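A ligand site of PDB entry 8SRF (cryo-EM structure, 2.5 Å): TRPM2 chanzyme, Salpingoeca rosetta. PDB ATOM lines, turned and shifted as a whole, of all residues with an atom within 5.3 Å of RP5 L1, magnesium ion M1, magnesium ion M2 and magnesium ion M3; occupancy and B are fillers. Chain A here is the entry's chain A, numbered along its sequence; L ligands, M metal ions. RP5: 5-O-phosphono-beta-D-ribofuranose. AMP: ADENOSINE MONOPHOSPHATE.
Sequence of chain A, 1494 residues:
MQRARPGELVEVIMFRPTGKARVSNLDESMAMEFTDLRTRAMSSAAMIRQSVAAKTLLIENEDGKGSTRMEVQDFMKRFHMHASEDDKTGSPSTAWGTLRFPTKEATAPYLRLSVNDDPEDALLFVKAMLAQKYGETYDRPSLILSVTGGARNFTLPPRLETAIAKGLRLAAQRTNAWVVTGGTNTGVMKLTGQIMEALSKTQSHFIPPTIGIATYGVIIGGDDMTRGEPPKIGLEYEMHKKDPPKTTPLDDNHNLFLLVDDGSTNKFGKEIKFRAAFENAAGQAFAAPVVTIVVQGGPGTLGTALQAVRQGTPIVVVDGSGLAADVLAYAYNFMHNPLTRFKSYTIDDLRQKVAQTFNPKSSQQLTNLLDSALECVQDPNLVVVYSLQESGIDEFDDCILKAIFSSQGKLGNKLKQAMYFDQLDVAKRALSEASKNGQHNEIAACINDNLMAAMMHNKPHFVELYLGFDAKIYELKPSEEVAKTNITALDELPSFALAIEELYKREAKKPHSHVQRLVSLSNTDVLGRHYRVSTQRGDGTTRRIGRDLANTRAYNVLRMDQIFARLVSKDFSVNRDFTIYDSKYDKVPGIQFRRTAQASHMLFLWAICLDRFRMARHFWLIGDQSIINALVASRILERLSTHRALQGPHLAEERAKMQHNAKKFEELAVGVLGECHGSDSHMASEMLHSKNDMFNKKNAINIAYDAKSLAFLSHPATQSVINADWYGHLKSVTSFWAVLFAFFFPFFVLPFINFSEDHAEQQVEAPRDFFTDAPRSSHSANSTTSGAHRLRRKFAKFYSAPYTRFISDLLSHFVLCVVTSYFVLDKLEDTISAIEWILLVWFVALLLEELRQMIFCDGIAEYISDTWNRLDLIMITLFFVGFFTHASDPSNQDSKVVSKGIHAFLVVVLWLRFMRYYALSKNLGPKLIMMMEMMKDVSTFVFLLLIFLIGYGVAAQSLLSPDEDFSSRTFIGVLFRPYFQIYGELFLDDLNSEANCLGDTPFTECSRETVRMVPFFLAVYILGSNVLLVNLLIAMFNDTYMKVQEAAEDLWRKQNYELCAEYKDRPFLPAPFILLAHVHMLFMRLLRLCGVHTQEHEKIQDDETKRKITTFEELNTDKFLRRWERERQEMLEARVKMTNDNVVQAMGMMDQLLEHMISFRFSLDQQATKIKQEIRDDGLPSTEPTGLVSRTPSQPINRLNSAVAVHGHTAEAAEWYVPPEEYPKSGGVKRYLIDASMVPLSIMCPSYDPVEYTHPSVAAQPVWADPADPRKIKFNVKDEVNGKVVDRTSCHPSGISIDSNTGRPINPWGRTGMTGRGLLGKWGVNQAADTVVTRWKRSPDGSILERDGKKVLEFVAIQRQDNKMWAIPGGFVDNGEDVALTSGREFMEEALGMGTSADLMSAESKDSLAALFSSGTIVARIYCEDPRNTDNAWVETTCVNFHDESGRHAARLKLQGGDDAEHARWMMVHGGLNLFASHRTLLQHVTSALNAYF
Magnesium ion M3 is bound by O3P of AMP L2 (2.1 Å) and OE2 of Glu 1386 (2.5 Å).
The side-chain carboxylate of Asp 1426 lies within salt-bridge range of the guanidinium group of Arg 1428. The backbone NH of Cys 1424 sits at hydrogen-bond distance from the backbone carbonyl oxygen of Val 1435 (3.2 Å). The backbone NH (N) of Ile 1368 sits at hydrogen-bond distance from a ring nitrogen (ND1) of His 1479 (3.2 Å). OE2 of Glu 1386 sits close to NH1 of Arg 1385 (2.6 Å). The backbone carbonyl oxygen (O) of Gly 1371 is in hydrogen-bond range of the backbone NH (N) of Ala 1329 (2.9 Å). The guanidinium group (NE) of Arg 1360 is in salt-bridge range of the side-chain carboxylate (OD1) of Asp 1362 (3.2 Å). A ring nitrogen (ND1) of His 1479 lies close to the backbone carbonyl oxygen (O) of Phe 1476. OD2 of Asp 1374 lies within salt-bridge range of NH2 of Arg 1385 (3.5 Å).
An oxygen (O1) of RP5 L1 is in hydrogen-bond range of the side-chain carboxylate (OD2) of Asp 1426, at 2.9 Å. An oxygen (O1) of RP5 L1 sits at hydrogen-bond distance from the side-chain sulfur (SG) of Cys 1424 (2.9 Å). O2 of RP5 L1 sits at hydrogen-bond distance from OD2 of Asp 1330, at 2.5 Å. O3 of RP5 L1 sits at hydrogen-bond distance from NE2 of His 1479 (3.0 Å). The guanidinium group (NH1) of Arg 1428 lies within salt-bridge range of an oxygen (O2X) of RP5 L1 (3.0 Å). The guanidinium group (NH2) of Arg 1360 lies within salt-bridge range of an oxygen (O2X) of RP5 L1 (2.6 Å).
Residues that only touch RP5 L1: Phe 1372 (3.3 Å), Phe 1476 (3.5 Å), Val 1435 (3.7 Å), Gly 1371 (3.7 Å), Ala 1328 (3.9 Å) and Thr 1437 (3.9 Å). Along chain A the residues within 4 Å of RP5 L1 span positions 1328 to 1479. The nearest printed residue that does not touch RP5 L1 is Ala 1477 (4.1 Å).
Merely in contact with magnesium ion M2: Asp 1459 (3.7 Å).
Magnesium ion M1 is bound by an oxygen (O1X) of RP5 L1 (2.1 Å), the side-chain carboxylate of Glu 1390 (2.1 Å), an oxygen (O2P) of AMP L2 (2.1 Å) and the side-chain carboxylate of Asp 1460 (2.3 Å). Magnesium ion M1 has four donor atoms within binding distance. Slightly farther from magnesium ion M1 lies the backbone carbonyl oxygen (O) of Gly 1370 (2.8 Å).
Magnesium ion M2 is bound by OE2 of Glu 1390, O1P of AMP L2, OE1 of Glu 1386, O2P of AMP L2 and OD1 of Asp 1460. Magnesium ion M2 has five donor atoms within binding distance.
The nearest printed residue that does not touch magnesium ion M1 is Glu 1386 (4.3 Å).
Residues that only touch magnesium ion M3: Arg 1385. Two residues have an atom within 4 Å of magnesium ion M3: Arg 1385 and Glu 1386. The nearest printed residue that does not touch magnesium ion M3 is Asp 1374 (4.4 Å).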
ATOM      1  N   ALA A1328     -25.808 -19.677 -10.496  1.00  0.00           N
ATOM      2  CA  ALA A1328     -26.503 -20.510 -11.452  1.00  0.00           C
ATOM      3  C   ALA A1328     -26.258 -21.954 -11.075  1.00  0.00           C
ATOM      4  O   ALA A1328     -25.218 -22.307 -10.516  1.00  0.00           O
ATOM      5  CB  ALA A1328     -26.031 -20.257 -12.887  1.00  0.00           C
ATOM      6  N   ALA A1329     -27.240 -22.782 -11.379  1.00  0.00           N
ATOM      7  CA  ALA A1329     -27.127 -24.213 -11.179  1.00  0.00           C
ATOM      8  C   ALA A1329     -27.302 -24.862 -12.536  1.00  0.00           C
ATOM      9  O   ALA A1329     -28.241 -24.541 -13.273  1.00  0.00           O
ATOM     10  CB  ALA A1329     -28.173 -24.737 -10.198  1.00  0.00           C
ATOM     11  N   ASP A1330     -26.353 -25.729 -12.885  1.00  0.00           N
ATOM     12  CA  ASP A1330     -26.410 -26.492 -14.122  1.00  0.00           C
ATOM     13  C   ASP A1330     -26.600 -27.965 -13.821  1.00  0.00           C
ATOM     14  O   ASP A1330     -26.025 -28.496 -12.860  1.00  0.00           O
ATOM     15  CB  ASP A1330     -25.166 -26.240 -14.957  1.00  0.00           C
ATOM     16  CG  ASP A1330     -25.076 -24.818 -15.398  1.00  0.00           C
ATOM     17  OD1 ASP A1330     -26.151 -24.284 -15.721  1.00  0.00           O
ATOM     18  OD2 ASP A1330     -23.987 -24.232 -15.408  1.00  0.00           O
ATOM     19  N   ARG A1360     -31.068 -22.858 -26.542  1.00  0.00           N
ATOM     20  CA  ARG A1360     -31.539 -21.674 -25.828  1.00  0.00           C
ATOM     21  C   ARG A1360     -32.446 -20.811 -26.699  1.00  0.00           C
ATOM     22  O   ARG A1360     -32.280 -20.745 -27.922  1.00  0.00           O
ATOM     23  CB  ARG A1360     -30.361 -20.854 -25.325  1.00  0.00           C
ATOM     24  CG  ARG A1360     -29.433 -21.621 -24.408  1.00  0.00           C
ATOM     25  CD  ARG A1360     -28.307 -20.739 -23.936  1.00  0.00           C
ATOM     26  NE  ARG A1360     -28.785 -19.480 -23.373  1.00  0.00           N
ATOM     27  CZ  ARG A1360     -29.138 -19.304 -22.100  1.00  0.00           C
ATOM     28  NH1 ARG A1360     -29.081 -20.294 -21.224  1.00  0.00           N
ATOM     29  NH2 ARG A1360     -29.549 -18.116 -21.703  1.00  0.00           N
ATOM     30  N   ASP A1362     -32.906 -17.458 -26.421  1.00  0.00           N
ATOM     31  CA  ASP A1362     -32.417 -16.109 -26.689  1.00  0.00           C
ATOM     32  C   ASP A1362     -31.345 -16.045 -27.787  1.00  0.00           C
ATOM     33  O   ASP A1362     -31.412 -15.173 -28.663  1.00  0.00           O
ATOM     34  CB  ASP A1362     -31.978 -15.434 -25.372  1.00  0.00           C
ATOM     35  CG  ASP A1362     -30.863 -16.179 -24.624  1.00  0.00           C
ATOM     36  OD1 ASP A1362     -30.405 -17.273 -25.020  1.00  0.00           O
ATOM     37  OD2 ASP A1362     -30.420 -15.644 -23.581  1.00  0.00           O
ATOM     38  N   ILE A1368     -26.087 -26.630 -21.633  1.00  0.00           N
ATOM     39  CA  ILE A1368     -26.508 -27.476 -20.516  1.00  0.00           C
ATOM     40  C   ILE A1368     -27.735 -26.815 -19.869  1.00  0.00           C
ATOM     41  O   ILE A1368     -27.798 -25.572 -19.868  1.00  0.00           O
ATOM     42  CB  ILE A1368     -25.351 -27.605 -19.511  1.00  0.00           C
ATOM     43  CG1 ILE A1368     -24.233 -28.465 -20.097  1.00  0.00           C
ATOM     44  CG2 ILE A1368     -25.735 -28.172 -18.168  1.00  0.00           C
ATOM     45  CD1 ILE A1368     -22.917 -28.350 -19.355  1.00  0.00           C
ATOM     46  N   GLY A1370     -30.158 -25.373 -17.086  1.00  0.00           N
ATOM     47  CA  GLY A1370     -29.830 -24.763 -15.812  1.00  0.00           C
ATOM     48  C   GLY A1370     -30.394 -23.366 -15.773  1.00  0.00           C
ATOM     49  O   GLY A1370     -30.932 -22.845 -16.753  1.00  0.00           O
ATOM     50  N   GLY A1371     -30.242 -22.755 -14.604  1.00  0.00           N
ATOM     51  CA  GLY A1371     -30.790 -21.433 -14.442  1.00  0.00           C
ATOM     52  C   GLY A1371     -30.350 -20.821 -13.138  1.00  0.00           C
ATOM     53  O   GLY A1371     -29.614 -21.444 -12.354  1.00  0.00           O
ATOM     54  N   PHE A1372     -30.728 -19.549 -12.973  1.00  0.00           N
ATOM     55  CA  PHE A1372     -30.352 -18.769 -11.805  1.00  0.00           C
ATOM     56  C   PHE A1372     -31.040 -19.272 -10.545  1.00  0.00           C
ATOM     57  O   PHE A1372     -32.191 -19.710 -10.574  1.00  0.00           O
ATOM     58  CB  PHE A1372     -30.665 -17.294 -12.052  1.00  0.00           C
ATOM     59  CG  PHE A1372     -29.847 -16.707 -13.144  1.00  0.00           C
ATOM     60  CD1 PHE A1372     -28.481 -16.440 -12.936  1.00  0.00           C
ATOM     61  CD2 PHE A1372     -30.413 -16.477 -14.406  1.00  0.00           C
ATOM     62  CE1 PHE A1372     -27.693 -15.895 -13.954  1.00  0.00           C
ATOM     63  CE2 PHE A1372     -29.637 -15.938 -15.452  1.00  0.00           C
ATOM     64  CZ  PHE A1372     -28.283 -15.650 -15.216  1.00  0.00           C
ATOM     65  N   ASP A1374     -33.043 -19.065  -7.341  1.00  0.00           N
ATOM     66  CA  ASP A1374     -34.092 -18.216  -6.798  1.00  0.00           C
ATOM     67  C   ASP A1374     -33.835 -17.936  -5.304  1.00  0.00           C
ATOM     68  O   ASP A1374     -33.020 -18.597  -4.651  1.00  0.00           O
ATOM     69  CB  ASP A1374     -35.455 -18.873  -6.985  1.00  0.00           C
ATOM     70  CG  ASP A1374     -36.021 -18.657  -8.374  1.00  0.00           C
ATOM     71  OD1 ASP A1374     -35.499 -17.778  -9.098  1.00  0.00           O
ATOM     72  OD2 ASP A1374     -36.979 -19.361  -8.746  1.00  0.00           O
ATOM     73  N   ARG A1385     -35.616 -28.400 -10.540  1.00  0.00           N
ATOM     74  CA  ARG A1385     -36.691 -27.553 -11.071  1.00  0.00           C
ATOM     75  C   ARG A1385     -36.393 -27.024 -12.468  1.00  0.00           C
ATOM     76  O   ARG A1385     -37.278 -27.058 -13.334  1.00  0.00           O
ATOM     77  CB  ARG A1385     -36.947 -26.397 -10.092  1.00  0.00           C
ATOM     78  CG  ARG A1385     -38.100 -25.471 -10.482  1.00  0.00           C
ATOM     79  CD  ARG A1385     -38.225 -24.313  -9.505  1.00  0.00           C
ATOM     80  NE  ARG A1385     -36.939 -23.703  -9.152  1.00  0.00           N
ATOM     81  CZ  ARG A1385     -36.307 -22.786  -9.867  1.00  0.00           C
ATOM     82  NH1 ARG A1385     -36.791 -22.328 -11.014  1.00  0.00           N
ATOM     83  NH2 ARG A1385     -35.156 -22.301  -9.426  1.00  0.00           N
ATOM     84  N   GLU A1386     -35.152 -26.546 -12.703  1.00  0.00           N
ATOM     85  CA  GLU A1386     -34.721 -26.059 -14.029  1.00  0.00           C
ATOM     86  C   GLU A1386     -34.641 -27.173 -15.051  1.00  0.00           C
ATOM     87  O   GLU A1386     -34.854 -26.909 -16.246  1.00  0.00           O
ATOM     88  CB  GLU A1386     -33.433 -25.239 -13.982  1.00  0.00           C
ATOM     89  CG  GLU A1386     -33.523 -23.831 -13.324  1.00  0.00           C
ATOM     90  CD  GLU A1386     -34.616 -22.908 -13.880  1.00  0.00           C
ATOM     91  OE1 GLU A1386     -34.813 -22.850 -15.108  1.00  0.00           O
ATOM     92  OE2 GLU A1386     -35.268 -22.223 -13.062  1.00  0.00           O
ATOM     93  N   GLU A1389     -38.290 -27.957 -15.875  1.00  0.00           N
ATOM     94  CA  GLU A1389     -38.866 -26.864 -16.665  1.00  0.00           C
ATOM     95  C   GLU A1389     -38.317 -26.788 -18.086  1.00  0.00           C
ATOM     96  O   GLU A1389     -39.066 -26.544 -19.032  1.00  0.00           O
ATOM     97  CB  GLU A1389     -38.699 -25.517 -15.958  1.00  0.00           C
ATOM     98  CG  GLU A1389     -39.702 -25.273 -14.834  1.00  0.00           C
ATOM     99  CD  GLU A1389     -39.318 -24.093 -13.964  1.00  0.00           C
ATOM    100  OE1 GLU A1389     -38.287 -23.446 -14.244  1.00  0.00           O
ATOM    101  OE2 GLU A1389     -40.057 -23.802 -13.004  1.00  0.00           O
ATOM    102  N   GLU A1390     -36.995 -26.940 -18.250  1.00  0.00           N
ATOM    103  CA  GLU A1390     -36.364 -26.713 -19.548  1.00  0.00           C
ATOM    104  C   GLU A1390     -36.277 -27.964 -20.406  1.00  0.00           C
ATOM    105  O   GLU A1390     -36.735 -27.940 -21.564  1.00  0.00           O
ATOM    106  CB  GLU A1390     -34.990 -26.090 -19.320  1.00  0.00           C
ATOM    107  CG  GLU A1390     -35.085 -24.678 -18.747  1.00  0.00           C
ATOM    108  CD  GLU A1390     -33.736 -24.040 -18.496  1.00  0.00           C
ATOM    109  OE1 GLU A1390     -32.714 -24.608 -18.913  1.00  0.00           O
ATOM    110  OE2 GLU A1390     -33.705 -22.962 -17.884  1.00  0.00           O
ATOM    111  N   CYS A1424     -18.425 -18.489 -14.786  1.00  0.00           N
ATOM    112  CA  CYS A1424     -18.960 -18.621 -16.128  1.00  0.00           C
ATOM    113  C   CYS A1424     -18.330 -17.610 -17.055  1.00  0.00           C
ATOM    114  O   CYS A1424     -18.153 -16.447 -16.695  1.00  0.00           O
ATOM    115  CB  CYS A1424     -20.468 -18.411 -16.208  1.00  0.00           C
ATOM    116  SG  CYS A1424     -21.514 -19.655 -15.561  1.00  0.00           S
ATOM    117  N   ASP A1426     -19.863 -16.169 -19.481  1.00  0.00           N
ATOM    118  CA  ASP A1426     -21.152 -15.742 -19.966  1.00  0.00           C
ATOM    119  C   ASP A1426     -21.040 -14.340 -20.562  1.00  0.00           C
ATOM    120  O   ASP A1426     -20.426 -13.470 -19.937  1.00  0.00           O
ATOM    121  CB  ASP A1426     -22.160 -15.759 -18.809  1.00  0.00           C
ATOM    122  CG  ASP A1426     -23.617 -15.684 -19.255  1.00  0.00           C
ATOM    123  OD1 ASP A1426     -24.094 -14.653 -19.753  1.00  0.00           O
ATOM    124  OD2 ASP A1426     -24.311 -16.680 -19.056  1.00  0.00           O
ATOM    125  N   ARG A1428     -23.207 -11.965 -20.883  1.00  0.00           N
ATOM    126  CA  ARG A1428     -23.994 -10.974 -20.156  1.00  0.00           C
ATOM    127  C   ARG A1428     -23.304 -10.446 -18.897  1.00  0.00           C
ATOM    128  O   ARG A1428     -23.926  -9.655 -18.189  1.00  0.00           O
ATOM    129  CB  ARG A1428     -25.347 -11.539 -19.718  1.00  0.00           C
ATOM    130  CG  ARG A1428     -26.181 -12.125 -20.816  1.00  0.00           C
ATOM    131  CD  ARG A1428     -27.277 -12.988 -20.227  1.00  0.00           C
ATOM    132  NE  ARG A1428     -26.734 -14.224 -19.670  1.00  0.00           N
ATOM    133  CZ  ARG A1428     -27.462 -15.186 -19.137  1.00  0.00           C
ATOM    134  NH1 ARG A1428     -28.781 -15.084 -19.054  1.00  0.00           N
ATOM    135  NH2 ARG A1428     -26.860 -16.273 -18.665  1.00  0.00           N
ATOM    136  N   VAL A1435     -22.046 -14.179 -13.513  1.00  0.00           N
ATOM    137  CA  VAL A1435     -22.662 -15.478 -13.276  1.00  0.00           C
ATOM    138  C   VAL A1435     -21.591 -16.461 -12.810  1.00  0.00           C
ATOM    139  O   VAL A1435     -20.511 -16.539 -13.414  1.00  0.00           O
ATOM    140  CB  VAL A1435     -23.351 -15.992 -14.555  1.00  0.00           C
ATOM    141  CG1 VAL A1435     -24.109 -17.273 -14.312  1.00  0.00           C
ATOM    142  CG2 VAL A1435     -24.277 -14.946 -15.101  1.00  0.00           C
ATOM    143  N   THR A1437     -21.324 -20.628 -11.588  1.00  0.00           N
ATOM    144  CA  THR A1437     -22.161 -21.819 -11.660  1.00  0.00           C
ATOM    145  C   THR A1437     -21.672 -22.910 -10.716  1.00  0.00           C
ATOM    146  O   THR A1437     -20.491 -22.994 -10.356  1.00  0.00           O
ATOM    147  CB  THR A1437     -22.254 -22.411 -13.094  1.00  0.00           C
ATOM    148  OG1 THR A1437     -23.050 -23.601 -13.047  1.00  0.00           O
ATOM    149  CG2 THR A1437     -20.893 -22.807 -13.677  1.00  0.00           C
ATOM    150  N   ASP A1459     -40.262 -23.821 -21.434  1.00  0.00           N
ATOM    151  CA  ASP A1459     -39.909 -22.550 -20.740  1.00  0.00           C
ATOM    152  C   ASP A1459     -38.930 -21.780 -21.621  1.00  0.00           C
ATOM    153  O   ASP A1459     -39.317 -21.380 -22.734  1.00  0.00           O
ATOM    154  CB  ASP A1459     -39.447 -22.870 -19.312  1.00  0.00           C
ATOM    155  CG  ASP A1459     -39.406 -21.642 -18.415  1.00  0.00           C
ATOM    156  OD1 ASP A1459     -40.055 -20.636 -18.760  1.00  0.00           O
ATOM    157  OD2 ASP A1459     -38.723 -21.677 -17.372  1.00  0.00           O
ATOM    158  N   ASP A1460     -37.686 -21.538 -21.194  1.00  0.00           N
ATOM    159  CA  ASP A1460     -36.729 -20.761 -21.973  1.00  0.00           C
ATOM    160  C   ASP A1460     -35.778 -21.660 -22.779  1.00  0.00           C
ATOM    161  O   ASP A1460     -34.634 -21.277 -23.032  1.00  0.00           O
ATOM    162  CB  ASP A1460     -35.969 -19.805 -21.041  1.00  0.00           C
ATOM    163  CG  ASP A1460     -35.166 -20.538 -19.975  1.00  0.00           C
ATOM    164  OD1 ASP A1460     -35.786 -21.166 -19.093  1.00  0.00           O
ATOM    165  OD2 ASP A1460     -33.920 -20.481 -20.013  1.00  0.00           O
ATOM    166  N   PHE A1476     -22.658 -22.819 -25.364  1.00  0.00           N
ATOM    167  CA  PHE A1476     -22.808 -21.489 -24.784  1.00  0.00           C
ATOM    168  C   PHE A1476     -21.969 -21.414 -23.510  1.00  0.00           C
ATOM    169  O   PHE A1476     -21.970 -22.364 -22.734  1.00  0.00           O
ATOM    170  CB  PHE A1476     -24.293 -21.249 -24.476  1.00  0.00           C
ATOM    171  CG  PHE A1476     -24.566 -20.046 -23.628  1.00  0.00           C
ATOM    172  CD1 PHE A1476     -24.339 -18.763 -24.137  1.00  0.00           C
ATOM    173  CD2 PHE A1476     -25.044 -20.197 -22.312  1.00  0.00           C
ATOM    174  CE1 PHE A1476     -24.592 -17.622 -23.358  1.00  0.00           C
ATOM    175  CE2 PHE A1476     -25.311 -19.074 -21.517  1.00  0.00           C
ATOM    176  CZ  PHE A1476     -25.083 -17.791 -22.050  1.00  0.00           C
ATOM    177  N   ALA A1477     -21.314 -20.263 -23.310  1.00  0.00           N
ATOM    178  CA  ALA A1477     -20.520 -19.811 -22.131  1.00  0.00           C
ATOM    179  C   ALA A1477     -19.380 -20.797 -21.860  1.00  0.00           C
ATOM    180  O   ALA A1477     -18.691 -21.201 -22.809  1.00  0.00           O
ATOM    181  CB  ALA A1477     -21.447 -19.542 -20.953  1.00  0.00           C
ATOM    182  N   HIS A1479     -19.571 -23.971 -20.720  1.00  0.00           N
ATOM    183  CA  HIS A1479     -20.148 -25.301 -20.527  1.00  0.00           C
ATOM    184  C   HIS A1479     -19.236 -26.442 -20.994  1.00  0.00           C
ATOM    185  O   HIS A1479     -19.438 -27.588 -20.550  1.00  0.00           O
ATOM    186  CB  HIS A1479     -21.496 -25.388 -21.237  1.00  0.00           C
ATOM    187  CG  HIS A1479     -22.574 -24.618 -20.551  1.00  0.00           C
ATOM    188  ND1 HIS A1479     -23.844 -24.481 -21.080  1.00  0.00           N
ATOM    189  CD2 HIS A1479     -22.590 -23.951 -19.376  1.00  0.00           C
ATOM    190  CE1 HIS A1479     -24.584 -23.750 -20.255  1.00  0.00           C
ATOM    191  NE2 HIS A1479     -23.850 -23.416 -19.216  1.00  0.00           N
ATOM    192  N   LEU A1482     -17.294 -27.348 -17.963  1.00  0.00           N
ATOM    193  CA  LEU A1482     -18.186 -28.141 -17.114  1.00  0.00           C
ATOM    194  C   LEU A1482     -18.276 -29.598 -17.566  1.00  0.00           C
ATOM    195  O   LEU A1482     -18.222 -30.502 -16.727  1.00  0.00           O
ATOM    196  CB  LEU A1482     -19.583 -27.520 -17.123  1.00  0.00           C
ATOM    197  CG  LEU A1482     -19.752 -26.142 -16.502  1.00  0.00           C
ATOM    198  CD1 LEU A1482     -21.204 -25.797 -16.549  1.00  0.00           C
ATOM    199  CD2 LEU A1482     -19.294 -26.162 -15.066  1.00  0.00           C
HETATM  200  C1  RP5 L   1     -24.590 -19.858 -17.843  1.00  0.00           C
HETATM  201  O4  RP5 L   1     -25.838 -19.071 -18.103  1.00  0.00           O
HETATM  202  C2  RP5 L   1     -25.000 -20.748 -16.582  1.00  0.00           C
HETATM  203  O2  RP5 L   1     -24.104 -21.951 -16.494  1.00  0.00           O
HETATM  204  C3  RP5 L   1     -26.165 -21.071 -16.844  1.00  0.00           C
HETATM  205  O3  RP5 L   1     -26.186 -22.356 -17.582  1.00  0.00           O
HETATM  206  C4  RP5 L   1     -26.807 -19.891 -17.819  1.00  0.00           C
HETATM  207  C5  RP5 L   1     -27.898 -19.190 -17.076  1.00  0.00           C
HETATM  208  O5  RP5 L   1     -29.099 -19.836 -17.367  1.00  0.00           O
HETATM  209  P'  RP5 L   1     -30.209 -19.010 -18.237  1.00  0.00           P
HETATM  210  O1X RP5 L   1     -31.022 -19.967 -19.065  1.00  0.00           O
HETATM  211  O2X RP5 L   1     -29.514 -18.030 -19.147  1.00  0.00           O
HETATM  212  O3X RP5 L   1     -31.105 -18.267 -17.288  1.00  0.00           O
HETATM  213  O1  RP5 L   1     -23.623 -19.090 -17.536  1.00  0.00           O
HETATM  214  P   AMP L   2     -34.217 -19.465 -15.744  1.00  0.00           P
HETATM  215  O1P AMP L   2     -35.623 -19.709 -16.218  1.00  0.00           O
HETATM  216  O2P AMP L   2     -33.276 -20.316 -16.562  1.00  0.00           O
HETATM  217  O3P AMP L   2     -34.191 -19.607 -14.245  1.00  0.00           O
HETATM  218  O5' AMP L   2     -33.830 -17.964 -16.087  1.00  0.00           O
HETATM  219  C5' AMP L   2     -34.361 -17.322 -17.227  1.00  0.00           C
HETATM  220  C4' AMP L   2     -35.140 -16.097 -16.836  1.00  0.00           C
HETATM  221  O4' AMP L   2     -35.339 -16.095 -15.397  1.00  0.00           O
HETATM  222  C3' AMP L   2     -34.476 -14.754 -17.105  1.00  0.00           C
HETATM  223  O3' AMP L   2     -34.594 -14.351 -18.455  1.00  0.00           O
HETATM  224  C2' AMP L   2     -35.178 -13.835 -16.125  1.00  0.00           C
HETATM  225  O2' AMP L   2     -36.458 -13.469 -16.601  1.00  0.00           O
HETATM  226  C1' AMP L   2     -35.354 -14.769 -14.913  1.00  0.00           C
HETATM  227  N9  AMP L   2     -34.329 -14.637 -13.853  1.00  0.00           N
HETATM  228  C8  AMP L   2     -34.538 -15.188 -12.659  1.00  0.00           C
HETATM  229  N7  AMP L   2     -33.493 -14.955 -11.860  1.00  0.00           N
HETATM  230  C5  AMP L   2     -32.610 -14.248 -12.571  1.00  0.00           C
HETATM  231  C6  AMP L   2     -31.370 -13.746 -12.247  1.00  0.00           C
HETATM  232  N6  AMP L   2     -30.568 -13.792 -11.035  1.00  0.00           N
HETATM  233  N1  AMP L   2     -30.639 -13.067 -13.115  1.00  0.00           N
HETATM  234  C2  AMP L   2     -31.094 -12.836 -14.371  1.00  0.00           C
HETATM  235  N3  AMP L   2     -32.316 -13.336 -14.679  1.00  0.00           N
HETATM  236  C4  AMP L   2     -33.099 -14.042 -13.811  1.00  0.00           C
HETATM  237 MG    MG M   1     -32.562 -21.236 -18.351  1.00  0.00          MG
HETATM  238 MG    MG M   2     -35.017 -21.643 -16.860  1.00  0.00          MG
HETATM  239 MG    MG M   3     -35.897 -19.776 -12.968  1.00  0.00          MG
